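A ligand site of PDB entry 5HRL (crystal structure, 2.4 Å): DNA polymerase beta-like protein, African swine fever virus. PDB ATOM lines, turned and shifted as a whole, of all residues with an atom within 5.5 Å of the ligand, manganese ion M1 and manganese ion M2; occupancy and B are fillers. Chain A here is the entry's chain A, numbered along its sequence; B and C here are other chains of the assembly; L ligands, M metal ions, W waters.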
ATOM      1  N   VAL A  41      -7.147 -23.360 -19.463  1.00  0.00           N
ATOM      2  CA  VAL A  41      -5.863 -23.523 -18.827  1.00  0.00           C
ATOM      3  C   VAL A  41      -4.879 -24.307 -19.736  1.00  0.00           C
ATOM      4  O   VAL A  41      -5.057 -24.364 -20.962  1.00  0.00           O
ATOM      5  CB  VAL A  41      -6.044 -24.108 -17.396  1.00  0.00           C
ATOM      6  CG1 VAL A  41      -6.763 -23.100 -16.487  1.00  0.00           C
ATOM      7  CG2 VAL A  41      -6.814 -25.401 -17.414  1.00  0.00           C
ATOM      8  N   GLY A  42      -3.795 -24.830 -19.182  1.00  0.00           N
ATOM      9  CA  GLY A  42      -2.796 -25.543 -19.968  1.00  0.00           C
ATOM     10  C   GLY A  42      -2.234 -24.766 -21.156  1.00  0.00           C
ATOM     11  O   GLY A  42      -2.196 -23.547 -21.189  1.00  0.00           O
ATOM     12  N   SER A  43      -1.792 -25.500 -22.154  1.00  0.00           N
ATOM     13  CA  SER A  43      -1.081 -24.904 -23.303  1.00  0.00           C
ATOM     14  C   SER A  43      -1.939 -23.984 -24.092  1.00  0.00           C
ATOM     15  O   SER A  43      -1.461 -22.996 -24.610  1.00  0.00           O
ATOM     16  CB  SER A  43      -0.510 -25.989 -24.227  1.00  0.00           C
ATOM     17  OG  SER A  43      -1.529 -26.903 -24.538  1.00  0.00           O
ATOM     18  N   LEU A  44      -3.230 -24.232 -24.125  1.00  0.00           N
ATOM     19  CA  LEU A  44      -4.113 -23.277 -24.699  1.00  0.00           C
ATOM     20  C   LEU A  44      -4.065 -21.903 -24.045  1.00  0.00           C
ATOM     21  O   LEU A  44      -4.016 -20.942 -24.724  1.00  0.00           O
ATOM     22  CB  LEU A  44      -5.520 -23.829 -24.764  1.00  0.00           C
ATOM     23  CG  LEU A  44      -6.669 -22.987 -25.269  1.00  0.00           C
ATOM     24  CD1 LEU A  44      -6.513 -22.595 -26.698  1.00  0.00           C
ATOM     25  CD2 LEU A  44      -7.988 -23.662 -25.062  1.00  0.00           C
ATOM     26  N   ARG A  46      -1.568 -20.826 -22.439  1.00  0.00           N
ATOM     27  CA  ARG A  46      -0.214 -20.336 -22.742  1.00  0.00           C
ATOM     28  C   ARG A  46      -0.008 -19.961 -24.223  1.00  0.00           C
ATOM     29  O   ARG A  46       1.078 -19.562 -24.614  1.00  0.00           O
ATOM     30  CB  ARG A  46       0.876 -21.290 -22.244  1.00  0.00           C
ATOM     31  CG  ARG A  46       0.895 -21.476 -20.717  1.00  0.00           C
ATOM     32  CD  ARG A  46       2.161 -22.163 -20.262  1.00  0.00           C
ATOM     33  NE  ARG A  46       2.518 -23.284 -21.137  1.00  0.00           N
ATOM     34  CZ  ARG A  46       2.069 -24.532 -21.026  1.00  0.00           C
ATOM     35  NH1 ARG A  46       1.251 -24.923 -20.036  1.00  0.00           N
ATOM     36  NH2 ARG A  46       2.456 -25.434 -21.915  1.00  0.00           N
ATOM     37  N   GLU A  48       0.251 -21.582 -26.970  1.00  0.00           N
ATOM     38  CA  GLU A  48       1.168 -22.379 -27.780  1.00  0.00           C
ATOM     39  C   GLU A  48       0.525 -22.697 -29.124  1.00  0.00           C
ATOM     40  O   GLU A  48      -0.679 -22.985 -29.227  1.00  0.00           O
ATOM     41  CB  GLU A  48       1.651 -23.631 -27.041  1.00  0.00           C
ATOM     42  CG  GLU A  48       3.056 -23.436 -26.510  1.00  0.00           C
ATOM     43  CD  GLU A  48       3.318 -24.165 -25.225  1.00  0.00           C
ATOM     44  OE1 GLU A  48       3.754 -23.509 -24.229  1.00  0.00           O
ATOM     45  OE2 GLU A  48       3.098 -25.384 -25.224  1.00  0.00           O
ATOM     46  N   MET A  50       0.696 -25.098 -31.241  1.00  0.00           N
ATOM     47  CA  MET A  50       0.034 -26.429 -31.284  1.00  0.00           C
ATOM     48  C   MET A  50      -0.288 -26.969 -29.892  1.00  0.00           C
ATOM     49  O   MET A  50       0.467 -26.759 -28.941  1.00  0.00           O
ATOM     50  CB  MET A  50       0.910 -27.443 -32.015  1.00  0.00           C
ATOM     51  CG  MET A  50       1.238 -27.087 -33.461  1.00  0.00           C
ATOM     52  SD  MET A  50      -0.263 -26.856 -34.448  1.00  0.00           S
ATOM     53  CE  MET A  50      -0.732 -28.549 -34.771  1.00  0.00           C
ATOM     54  N   LEU A  51      -1.401 -27.703 -29.787  1.00  0.00           N
ATOM     55  CA  LEU A  51      -1.871 -28.266 -28.514  1.00  0.00           C
ATOM     56  C   LEU A  51      -2.107 -29.775 -28.664  1.00  0.00           C
ATOM     57  O   LEU A  51      -2.572 -30.214 -29.714  1.00  0.00           O
ATOM     58  CB  LEU A  51      -3.219 -27.635 -28.145  1.00  0.00           C
ATOM     59  CG  LEU A  51      -3.450 -26.128 -28.352  1.00  0.00           C
ATOM     60  CD1 LEU A  51      -4.926 -25.813 -28.212  1.00  0.00           C
ATOM     61  CD2 LEU A  51      -2.650 -25.311 -27.335  1.00  0.00           C
ATOM     62  N   ASN A  52      -1.854 -30.550 -27.616  1.00  0.00           N
ATOM     63  CA  ASN A  52      -2.307 -31.977 -27.585  1.00  0.00           C
ATOM     64  C   ASN A  52      -3.750 -32.174 -27.145  1.00  0.00           C
ATOM     65  O   ASN A  52      -4.318 -33.253 -27.356  1.00  0.00           O
ATOM     66  CB  ASN A  52      -1.450 -32.794 -26.645  1.00  0.00           C
ATOM     67  CG  ASN A  52       0.005 -32.814 -27.056  1.00  0.00           C
ATOM     68  OD1 ASN A  52       0.370 -33.415 -28.084  1.00  0.00           O
ATOM     69  ND2 ASN A  52       0.848 -32.144 -26.253  1.00  0.00           N
ATOM     70  N   ASP A  53      -4.338 -31.174 -26.508  1.00  0.00           N
ATOM     71  CA  ASP A  53      -5.645 -31.322 -25.863  1.00  0.00           C
ATOM     72  C   ASP A  53      -6.143 -29.983 -25.415  1.00  0.00           C
ATOM     73  O   ASP A  53      -5.422 -28.978 -25.474  1.00  0.00           O
ATOM     74  CB  ASP A  53      -5.549 -32.240 -24.639  1.00  0.00           C
ATOM     75  CG  ASP A  53      -4.441 -31.817 -23.661  1.00  0.00           C
ATOM     76  OD1 ASP A  53      -4.565 -30.720 -23.038  1.00  0.00           O
ATOM     77  OD2 ASP A  53      -3.445 -32.583 -23.536  1.00  0.00           O
ATOM     78  N   VAL A  54      -7.398 -29.955 -24.984  1.00  0.00           N
ATOM     79  CA  VAL A  54      -7.991 -28.747 -24.427  1.00  0.00           C
ATOM     80  C   VAL A  54      -8.234 -28.936 -22.918  1.00  0.00           C
ATOM     81  O   VAL A  54      -8.860 -29.904 -22.495  1.00  0.00           O
ATOM     82  CB  VAL A  54      -9.301 -28.419 -25.158  1.00  0.00           C
ATOM     83  CG1 VAL A  54      -9.909 -27.156 -24.607  1.00  0.00           C
ATOM     84  CG2 VAL A  54      -9.031 -28.245 -26.657  1.00  0.00           C
ATOM     85  N   ASP A  55      -7.718 -28.003 -22.126  1.00  0.00           N
ATOM     86  CA  ASP A  55      -7.770 -28.095 -20.676  1.00  0.00           C
ATOM     87  C   ASP A  55      -8.660 -26.996 -20.123  1.00  0.00           C
ATOM     88  O   ASP A  55      -8.379 -25.810 -20.290  1.00  0.00           O
ATOM     89  CB  ASP A  55      -6.352 -27.949 -20.074  1.00  0.00           C
ATOM     90  CG  ASP A  55      -5.376 -29.027 -20.571  1.00  0.00           C
ATOM     91  OD1 ASP A  55      -5.559 -30.197 -20.199  1.00  0.00           O
ATOM     92  OD2 ASP A  55      -4.429 -28.712 -21.341  1.00  0.00           O
ATOM     93  N   GLN A 102      -9.180 -34.331 -27.531  1.00  0.00           N
ATOM     94  CA  GLN A 102      -9.147 -34.640 -26.109  1.00  0.00           C
ATOM     95  C   GLN A 102      -9.440 -33.408 -25.259  1.00  0.00           C
ATOM     96  O   GLN A 102      -8.689 -32.421 -25.295  1.00  0.00           O
ATOM     97  CB  GLN A 102      -7.789 -35.238 -25.732  1.00  0.00           C
ATOM     98  CG  GLN A 102      -7.808 -35.957 -24.395  1.00  0.00           C
ATOM     99  CD  GLN A 102      -6.461 -36.481 -24.000  1.00  0.00           C
ATOM    100  OE1 GLN A 102      -6.007 -37.506 -24.485  1.00  0.00           O
ATOM    101  NE2 GLN A 102      -5.825 -35.814 -23.075  1.00  0.00           N
ATOM    102  N   ASP A 104      -9.812 -32.129 -21.449  1.00  0.00           N
ATOM    103  CA  ASP A 104      -9.557 -32.386 -20.038  1.00  0.00           C
ATOM    104  C   ASP A 104     -10.312 -31.351 -19.202  1.00  0.00           C
ATOM    105  O   ASP A 104     -10.136 -30.138 -19.418  1.00  0.00           O
ATOM    106  CB  ASP A 104      -8.079 -32.194 -19.687  1.00  0.00           C
ATOM    107  CG  ASP A 104      -7.136 -33.128 -20.427  1.00  0.00           C
ATOM    108  OD1 ASP A 104      -7.574 -34.223 -20.827  1.00  0.00           O
ATOM    109  OD2 ASP A 104      -5.939 -32.759 -20.589  1.00  0.00           O
ATOM    110  N   PHE A 106     -11.122 -30.000 -15.178  1.00  0.00           N
ATOM    111  CA  PHE A 106     -10.752 -30.034 -13.773  1.00  0.00           C
ATOM    112  C   PHE A 106     -11.713 -29.175 -12.965  1.00  0.00           C
ATOM    113  O   PHE A 106     -12.423 -28.335 -13.518  1.00  0.00           O
ATOM    114  CB  PHE A 106      -9.322 -29.542 -13.575  1.00  0.00           C
ATOM    115  CG  PHE A 106      -8.326 -30.180 -14.521  1.00  0.00           C
ATOM    116  CD1 PHE A 106      -8.062 -29.615 -15.764  1.00  0.00           C
ATOM    117  CD2 PHE A 106      -7.646 -31.323 -14.170  1.00  0.00           C
ATOM    118  CE1 PHE A 106      -7.150 -30.183 -16.642  1.00  0.00           C
ATOM    119  CE2 PHE A 106      -6.736 -31.882 -15.031  1.00  0.00           C
ATOM    120  CZ  PHE A 106      -6.481 -31.323 -16.272  1.00  0.00           C
ATOM    121  N   HIS A 119      -1.605 -23.504 -11.057  1.00  0.00           N
ATOM    122  CA  HIS A 119      -1.204 -24.894 -11.212  1.00  0.00           C
ATOM    123  C   HIS A 119      -1.513 -25.412 -12.642  1.00  0.00           C
ATOM    124  O   HIS A 119      -0.657 -26.017 -13.285  1.00  0.00           O
ATOM    125  CB  HIS A 119      -1.992 -25.682 -10.180  1.00  0.00           C
ATOM    126  CG  HIS A 119      -1.947 -27.164 -10.322  1.00  0.00           C
ATOM    127  ND1 HIS A 119      -0.924 -27.926  -9.792  1.00  0.00           N
ATOM    128  CD2 HIS A 119      -2.842 -28.034 -10.830  1.00  0.00           C
ATOM    129  CE1 HIS A 119      -1.179 -29.200 -10.004  1.00  0.00           C
ATOM    130  NE2 HIS A 119      -2.335 -29.303 -10.640  1.00  0.00           N
ATOM    131  N   PHE A 120      -2.731 -25.182 -13.113  1.00  0.00           N
ATOM    132  CA  PHE A 120      -3.198 -25.797 -14.335  1.00  0.00           C
ATOM    133  C   PHE A 120      -2.778 -25.056 -15.600  1.00  0.00           C
ATOM    134  O   PHE A 120      -2.810 -25.627 -16.691  1.00  0.00           O
ATOM    135  CB  PHE A 120      -4.706 -25.948 -14.306  1.00  0.00           C
ATOM    136  CG  PHE A 120      -5.162 -27.117 -13.495  1.00  0.00           C
ATOM    137  CD1 PHE A 120      -4.808 -28.407 -13.874  1.00  0.00           C
ATOM    138  CD2 PHE A 120      -5.930 -26.933 -12.355  1.00  0.00           C
ATOM    139  CE1 PHE A 120      -5.239 -29.495 -13.133  1.00  0.00           C
ATOM    140  CE2 PHE A 120      -6.345 -28.006 -11.610  1.00  0.00           C
ATOM    141  CZ  PHE A 120      -6.013 -29.300 -11.988  1.00  0.00           C
ATOM    142  N   THR A 121      -2.365 -23.816 -15.454  1.00  0.00           N
ATOM    143  CA  THR A 121      -1.763 -23.043 -16.534  1.00  0.00           C
ATOM    144  C   THR A 121      -0.398 -23.594 -16.964  1.00  0.00           C
ATOM    145  O   THR A 121      -0.035 -23.510 -18.116  1.00  0.00           O
ATOM    146  CB  THR A 121      -1.596 -21.587 -16.086  1.00  0.00           C
ATOM    147  OG1 THR A 121      -2.894 -20.993 -15.995  1.00  0.00           O
ATOM    148  CG2 THR A 121      -0.743 -20.807 -17.028  1.00  0.00           C
ATOM    149  N   GLY A 122       0.370 -24.129 -16.027  1.00  0.00           N
ATOM    150  CA  GLY A 122       1.671 -24.666 -16.314  1.00  0.00           C
ATOM    151  C   GLY A 122       2.685 -23.614 -16.687  1.00  0.00           C
ATOM    152  O   GLY A 122       2.533 -22.444 -16.338  1.00  0.00           O
ATOM    153  N   PRO A 123       3.743 -24.015 -17.394  1.00  0.00           N
ATOM    154  CA  PRO A 123       4.054 -25.388 -17.781  1.00  0.00           C
ATOM    155  C   PRO A 123       4.573 -26.135 -16.580  1.00  0.00           C
ATOM    156  O   PRO A 123       4.892 -25.514 -15.547  1.00  0.00           O
ATOM    157  CB  PRO A 123       5.155 -25.217 -18.820  1.00  0.00           C
ATOM    158  CG  PRO A 123       5.835 -23.963 -18.447  1.00  0.00           C
ATOM    159  CD  PRO A 123       4.776 -23.071 -17.857  1.00  0.00           C
ATOM    160  N   VAL A 124       4.674 -27.442 -16.699  1.00  0.00           N
ATOM    161  CA  VAL A 124       5.060 -28.253 -15.561  1.00  0.00           C
ATOM    162  C   VAL A 124       6.405 -27.828 -15.015  1.00  0.00           C
ATOM    163  O   VAL A 124       6.577 -27.670 -13.828  1.00  0.00           O
ATOM    164  CB  VAL A 124       5.115 -29.735 -15.936  1.00  0.00           C
ATOM    165  CG1 VAL A 124       5.617 -30.558 -14.766  1.00  0.00           C
ATOM    166  CG2 VAL A 124       3.759 -30.210 -16.358  1.00  0.00           C
ATOM    167  N   LEU A 127       6.072 -25.001 -12.723  1.00  0.00           N
ATOM    168  CA  LEU A 127       5.501 -25.400 -11.441  1.00  0.00           C
ATOM    169  C   LEU A 127       6.561 -25.975 -10.551  1.00  0.00           C
ATOM    170  O   LEU A 127       6.630 -25.671  -9.359  1.00  0.00           O
ATOM    171  CB  LEU A 127       4.409 -26.465 -11.609  1.00  0.00           C
ATOM    172  CG  LEU A 127       3.159 -26.008 -12.330  1.00  0.00           C
ATOM    173  CD1 LEU A 127       2.095 -27.081 -12.188  1.00  0.00           C
ATOM    174  CD2 LEU A 127       2.661 -24.677 -11.799  1.00  0.00           C
ATOM    175  P    DG B   9      11.510 -31.599  -5.587  1.00  0.00           P
ATOM    176  OP1  DG B   9      11.545 -31.767  -4.100  1.00  0.00           O
ATOM    177  OP2  DG B   9      11.099 -32.735  -6.434  1.00  0.00           O
ATOM    178  O5'  DG B   9      10.694 -30.246  -5.777  1.00  0.00           O
ATOM    179  C5'  DG B   9       9.772 -30.022  -6.826  1.00  0.00           C
ATOM    180  C4'  DG B   9       8.516 -29.445  -6.217  1.00  0.00           C
ATOM    181  O4'  DG B   9       7.441 -29.539  -7.173  1.00  0.00           O
ATOM    182  C3'  DG B   9       8.022 -30.219  -5.000  1.00  0.00           C
ATOM    183  O3'  DG B   9       7.177 -29.388  -4.209  1.00  0.00           O
ATOM    184  C2'  DG B   9       7.252 -31.363  -5.640  1.00  0.00           C
ATOM    185  C1'  DG B   9       6.710 -30.733  -6.932  1.00  0.00           C
ATOM    186  N9   DG B   9       6.827 -31.579  -8.117  1.00  0.00           N
ATOM    187  C8   DG B   9       7.903 -32.356  -8.492  1.00  0.00           C
ATOM    188  N7   DG B   9       7.685 -33.019  -9.593  1.00  0.00           N
ATOM    189  C5   DG B   9       6.392 -32.654  -9.971  1.00  0.00           C
ATOM    190  C6   DG B   9       5.624 -33.053 -11.077  1.00  0.00           C
ATOM    191  O6   DG B   9       5.926 -33.828 -11.994  1.00  0.00           O
ATOM    192  N1   DG B   9       4.370 -32.445 -11.076  1.00  0.00           N
ATOM    193  C2   DG B   9       3.927 -31.567 -10.126  1.00  0.00           C
ATOM    194  N2   DG B   9       2.675 -31.089 -10.298  1.00  0.00           N
ATOM    195  N3   DG B   9       4.641 -31.183  -9.087  1.00  0.00           N
ATOM    196  C4   DG B   9       5.857 -31.764  -9.060  1.00  0.00           C
ATOM    197  P    DT B  10       6.643 -29.919  -2.791  1.00  0.00           P
ATOM    198  OP1  DT B  10       6.524 -28.741  -1.893  1.00  0.00           O
ATOM    199  OP2  DT B  10       7.444 -31.104  -2.417  1.00  0.00           O
ATOM    200  O5'  DT B  10       5.169 -30.433  -3.085  1.00  0.00           O
ATOM    201  C5'  DT B  10       4.137 -29.503  -3.463  1.00  0.00           C
ATOM    202  C4'  DT B  10       2.928 -30.249  -3.969  1.00  0.00           C
ATOM    203  O4'  DT B  10       3.273 -30.950  -5.186  1.00  0.00           O
ATOM    204  C3'  DT B  10       2.384 -31.316  -3.006  1.00  0.00           C
ATOM    205  O3'  DT B  10       1.060 -30.948  -2.583  1.00  0.00           O
ATOM    206  C2'  DT B  10       2.415 -32.608  -3.825  1.00  0.00           C
ATOM    207  C1'  DT B  10       2.429 -32.080  -5.236  1.00  0.00           C
ATOM    208  N1   DT B  10       2.940 -32.994  -6.272  1.00  0.00           N
ATOM    209  C2   DT B  10       2.169 -33.198  -7.385  1.00  0.00           C
ATOM    210  O2   DT B  10       1.100 -32.629  -7.568  1.00  0.00           O
ATOM    211  N3   DT B  10       2.682 -34.093  -8.296  1.00  0.00           N
ATOM    212  C4   DT B  10       3.887 -34.760  -8.206  1.00  0.00           C
ATOM    213  O4   DT B  10       4.224 -35.528  -9.111  1.00  0.00           O
ATOM    214  C5   DT B  10       4.640 -34.519  -7.002  1.00  0.00           C
ATOM    215  C7   DT B  10       5.949 -35.215  -6.818  1.00  0.00           C
ATOM    216  C6   DT B  10       4.147 -33.658  -6.105  1.00  0.00           C
ATOM    217  P    DA C   9      -2.244 -36.806 -18.621  1.00  0.00           P
ATOM    218  OP1  DA C   9      -3.252 -37.754 -19.150  1.00  0.00           O
ATOM    219  OP2  DA C   9      -1.120 -36.320 -19.453  1.00  0.00           O
ATOM    220  O5'  DA C   9      -3.051 -35.556 -18.053  1.00  0.00           O
ATOM    221  C5'  DA C   9      -2.360 -34.391 -17.579  1.00  0.00           C
ATOM    222  C4'  DA C   9      -3.088 -33.793 -16.402  1.00  0.00           C
ATOM    223  O4'  DA C   9      -3.087 -34.724 -15.307  1.00  0.00           O
ATOM    224  C3'  DA C   9      -2.463 -32.512 -15.858  1.00  0.00           C
ATOM    225  C2'  DA C   9      -2.745 -32.602 -14.369  1.00  0.00           C
ATOM    226  C1'  DA C   9      -2.642 -34.091 -14.119  1.00  0.00           C
ATOM    227  N9   DA C   9      -1.304 -34.580 -13.821  1.00  0.00           N
ATOM    228  C8   DA C   9      -0.512 -35.399 -14.590  1.00  0.00           C
ATOM    229  N7   DA C   9       0.627 -35.716 -14.030  1.00  0.00           N
ATOM    230  C5   DA C   9       0.584 -35.065 -12.797  1.00  0.00           C
ATOM    231  C6   DA C   9       1.478 -35.015 -11.729  1.00  0.00           C
ATOM    232  N6   DA C   9       2.665 -35.631 -11.722  1.00  0.00           N
ATOM    233  N1   DA C   9       1.128 -34.291 -10.636  1.00  0.00           N
ATOM    234  C2   DA C   9      -0.065 -33.667 -10.647  1.00  0.00           C
ATOM    235  N3   DA C   9      -0.996 -33.661 -11.591  1.00  0.00           N
ATOM    236  C4   DA C   9      -0.615 -34.381 -12.648  1.00  0.00           C
HETATM  237  P1  LIG L   1      -0.036 -30.012 -23.887  1.00  0.00           P
HETATM  238  O1  LIG L   1       1.074 -31.002 -23.795  1.00  0.00           O
HETATM  239  O2  LIG L   1      -1.376 -30.521 -23.417  1.00  0.00           O
HETATM  240  O3  LIG L   1      -0.109 -29.222 -25.191  1.00  0.00           O
HETATM  241  O4  LIG L   1       0.537 -28.958 -22.801  1.00  0.00           O
HETATM  242  P2  LIG L   1      -0.136 -28.710 -21.323  1.00  0.00           P
HETATM  243  O5  LIG L   1       0.957 -27.827 -20.785  1.00  0.00           O
HETATM  244  O6  LIG L   1      -1.544 -28.431 -21.706  1.00  0.00           O
HETATM  245  O7  LIG L   1      -0.066 -30.108 -20.606  1.00  0.00           O
HETATM  246  P3  LIG L   1      -1.196 -31.079 -20.052  1.00  0.00           P
HETATM  247  O8  LIG L   1      -0.383 -32.331 -19.833  1.00  0.00           O
HETATM  248  O9  LIG L   1      -2.475 -31.017 -20.817  1.00  0.00           O
HETATM  249  O10 LIG L   1      -1.447 -30.580 -18.511  1.00  0.00           O
HETATM  250  C1  LIG L   1      -2.292 -29.460 -18.299  1.00  0.00           C
HETATM  251  C2  LIG L   1      -1.781 -28.676 -17.122  1.00  0.00           C
HETATM  252  O11 LIG L   1      -1.865 -29.426 -15.890  1.00  0.00           O
HETATM  253  C3  LIG L   1      -0.329 -28.240 -17.219  1.00  0.00           C
HETATM  254  O12 LIG L   1      -0.096 -27.193 -18.186  1.00  0.00           O
HETATM  255  C4  LIG L   1      -0.036 -27.877 -15.737  1.00  0.00           C
HETATM  256  C5  LIG L   1      -0.947 -28.845 -14.979  1.00  0.00           C
HETATM  257  N1  LIG L   1      -0.072 -29.813 -14.321  1.00  0.00           N
HETATM  258  C6  LIG L   1       0.250 -29.757 -13.010  1.00  0.00           C
HETATM  259  N2  LIG L   1       1.120 -30.734 -12.674  1.00  0.00           N
HETATM  260  C7  LIG L   1       1.382 -31.426 -13.782  1.00  0.00           C
HETATM  261  C8  LIG L   1       2.241 -32.554 -14.123  1.00  0.00           C
HETATM  262  O13 LIG L   1       2.915 -33.068 -13.208  1.00  0.00           O
HETATM  263  N3  LIG L   1       2.244 -33.002 -15.393  1.00  0.00           N
HETATM  264  C9  LIG L   1       1.510 -32.410 -16.331  1.00  0.00           C
HETATM  265  N4  LIG L   1       1.544 -32.835 -17.608  1.00  0.00           N
HETATM  266  N5  LIG L   1       0.716 -31.348 -16.073  1.00  0.00           N
HETATM  267  C10 LIG L   1       0.607 -30.820 -14.855  1.00  0.00           C
HETATM  268 MN    MN M   1      -2.943 -29.758 -22.342  1.00  0.00          MN
HETATM  269 MN    MN M   2      -4.270 -31.732 -20.143  1.00  0.00          MN
HETATM  270  O   HOH W   1       3.430 -28.523 -19.275  1.00  0.00           O
HETATM  271  O   HOH W   2      -3.383 -28.358 -23.743  1.00  0.00           O
HETATM  272  O   HOH W   3      -2.202 -33.960 -21.010  1.00  0.00           O
HETATM  273  O   HOH W   4      -0.915 -33.031 -23.026  1.00  0.00           O
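The backbone NH (N) of Asn 52 lies within hydrogen-bond range of an oxygen (O3) of the ligand (3.3 Å). An oxygen (O5) of the ligand lies within salt-bridge range of the guanidinium group of Arg 46 (3.0 Å). N7 of DA 9 of chain C lies within hydrogen-bond range of N3 of the ligand (3.4 Å). The side-chain hydroxyl (OG) of Ser 43 is in hydrogen-bond range of an oxygen (O3) of the ligand (2.8 Å). N of Ser 43 sits close to O6 of the ligand, 3.0 Å away. The side-chain amide nitrogen (ND2) of Asn 52 is in hydrogen-bond range of an oxygen (O1) of the ligand (2.7 Å). O13 of the ligand lies close to N1 of DG 9 of chain B. O12 of the ligand sits close to O of Phe 120 (3.5 Å).
The backbone carbonyl oxygen (O) of Thr 121 is in hydrogen-bond range of the guanidinium group (NH1) of Arg 46 (2.7 Å). The backbone carbonyl oxygen (O) of Asp 55 sits at hydrogen-bond distance from the backbone NH (N) of Val 41 (2.9 Å). The backbone NH of Gly 42 is in hydrogen-bond range of the backbone carbonyl oxygen of Phe 120 (2.8 Å). The backbone NH of Asp 104 sits at hydrogen-bond distance from the backbone carbonyl oxygen of Val 54, at 2.6 Å. The guanidinium group (NH2) of Arg 46 lies within salt-bridge range of the side-chain carboxylate (OE1) of Glu 48. The backbone NH of Glu 48 sits at hydrogen-bond distance from the backbone carbonyl oxygen of Ser 43, at 3.2 Å. The side-chain carboxylate (OD1) of Asp 104 sits at hydrogen-bond distance from the side-chain amide nitrogen (NE2) of Gln 102 (3.3 Å).
CA of Gly 42 touches O6 of the ligand, 3.6 Å away. CA of Leu 51 touches O3 of the ligand, at 3.9 Å. His 119 touches the ligand (O to C4, 3.1 Å). Thr 121 touches the ligand (O to O12, 3.7 Å). Gly 122 touches the ligand. CG2 of Val 124 touches C9 of the ligand (3.1 Å). CD1 of Leu 127 touches C6 of the ligand (3.4 Å). Hydrophobic or aromatic side chains within 4 Å of the ligand: His 119, Phe 120, Val 124 and Leu 127.
Merely in contact with manganese ion M1: Ser 43 (3.9 Å). Within 4 Å of manganese ion M1: Ser 43, Asp 53 and Asp 55. The nearest printed residue that does not touch manganese ion M1 is Asp 104 (4.6 Å).
Three residues have an atom within 4 Å of manganese ion M2: Asp 53, Asp 55 and Asp 104. The nearest printed residue that does not touch manganese ion M2 is DA 9 of chain C (4.2 Å).
Manganese ion M1 is bound by OD1 of Asp 53 (2.0 Å), water W2 (2.0 Å), O6 of the ligand (2.0 Å), O9 of the ligand (2.0 Å), O2 of the ligand (2.0 Å) and OD2 of Asp 55 (2.1 Å). Manganese ion M1 has six donor atoms within binding distance.
Manganese ion M2 is bound by OD1 of Asp 55 (2.0 Å), OD2 of Asp 104 (2.0 Å) and O9 of the ligand (2.0 Å). Manganese ion M2 has three donor atoms within binding distance.
Water W2 bridges the side-chain hydroxyl (OG) of Ser 43 (2.5 Å) and the backbone carbonyl oxygen (O) of Asp 53 (2.7 Å). Water W4 lies within hydrogen-bond range of the side-chain carboxylate (OD2) of Asp 53 and an oxygen (O1) of the ligand. Water W3 lies within hydrogen-bond range of an oxygen (O8) of the ligand (2.7 Å), OP2 of DA 9 of chain C (3.0 Å) and the side-chain carboxylate of Asp 53 (3.1 Å). Water W1 lies within hydrogen-bond range of O5 of the ligand (3.0 Å) and N of Val 124 (3.1 Å).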
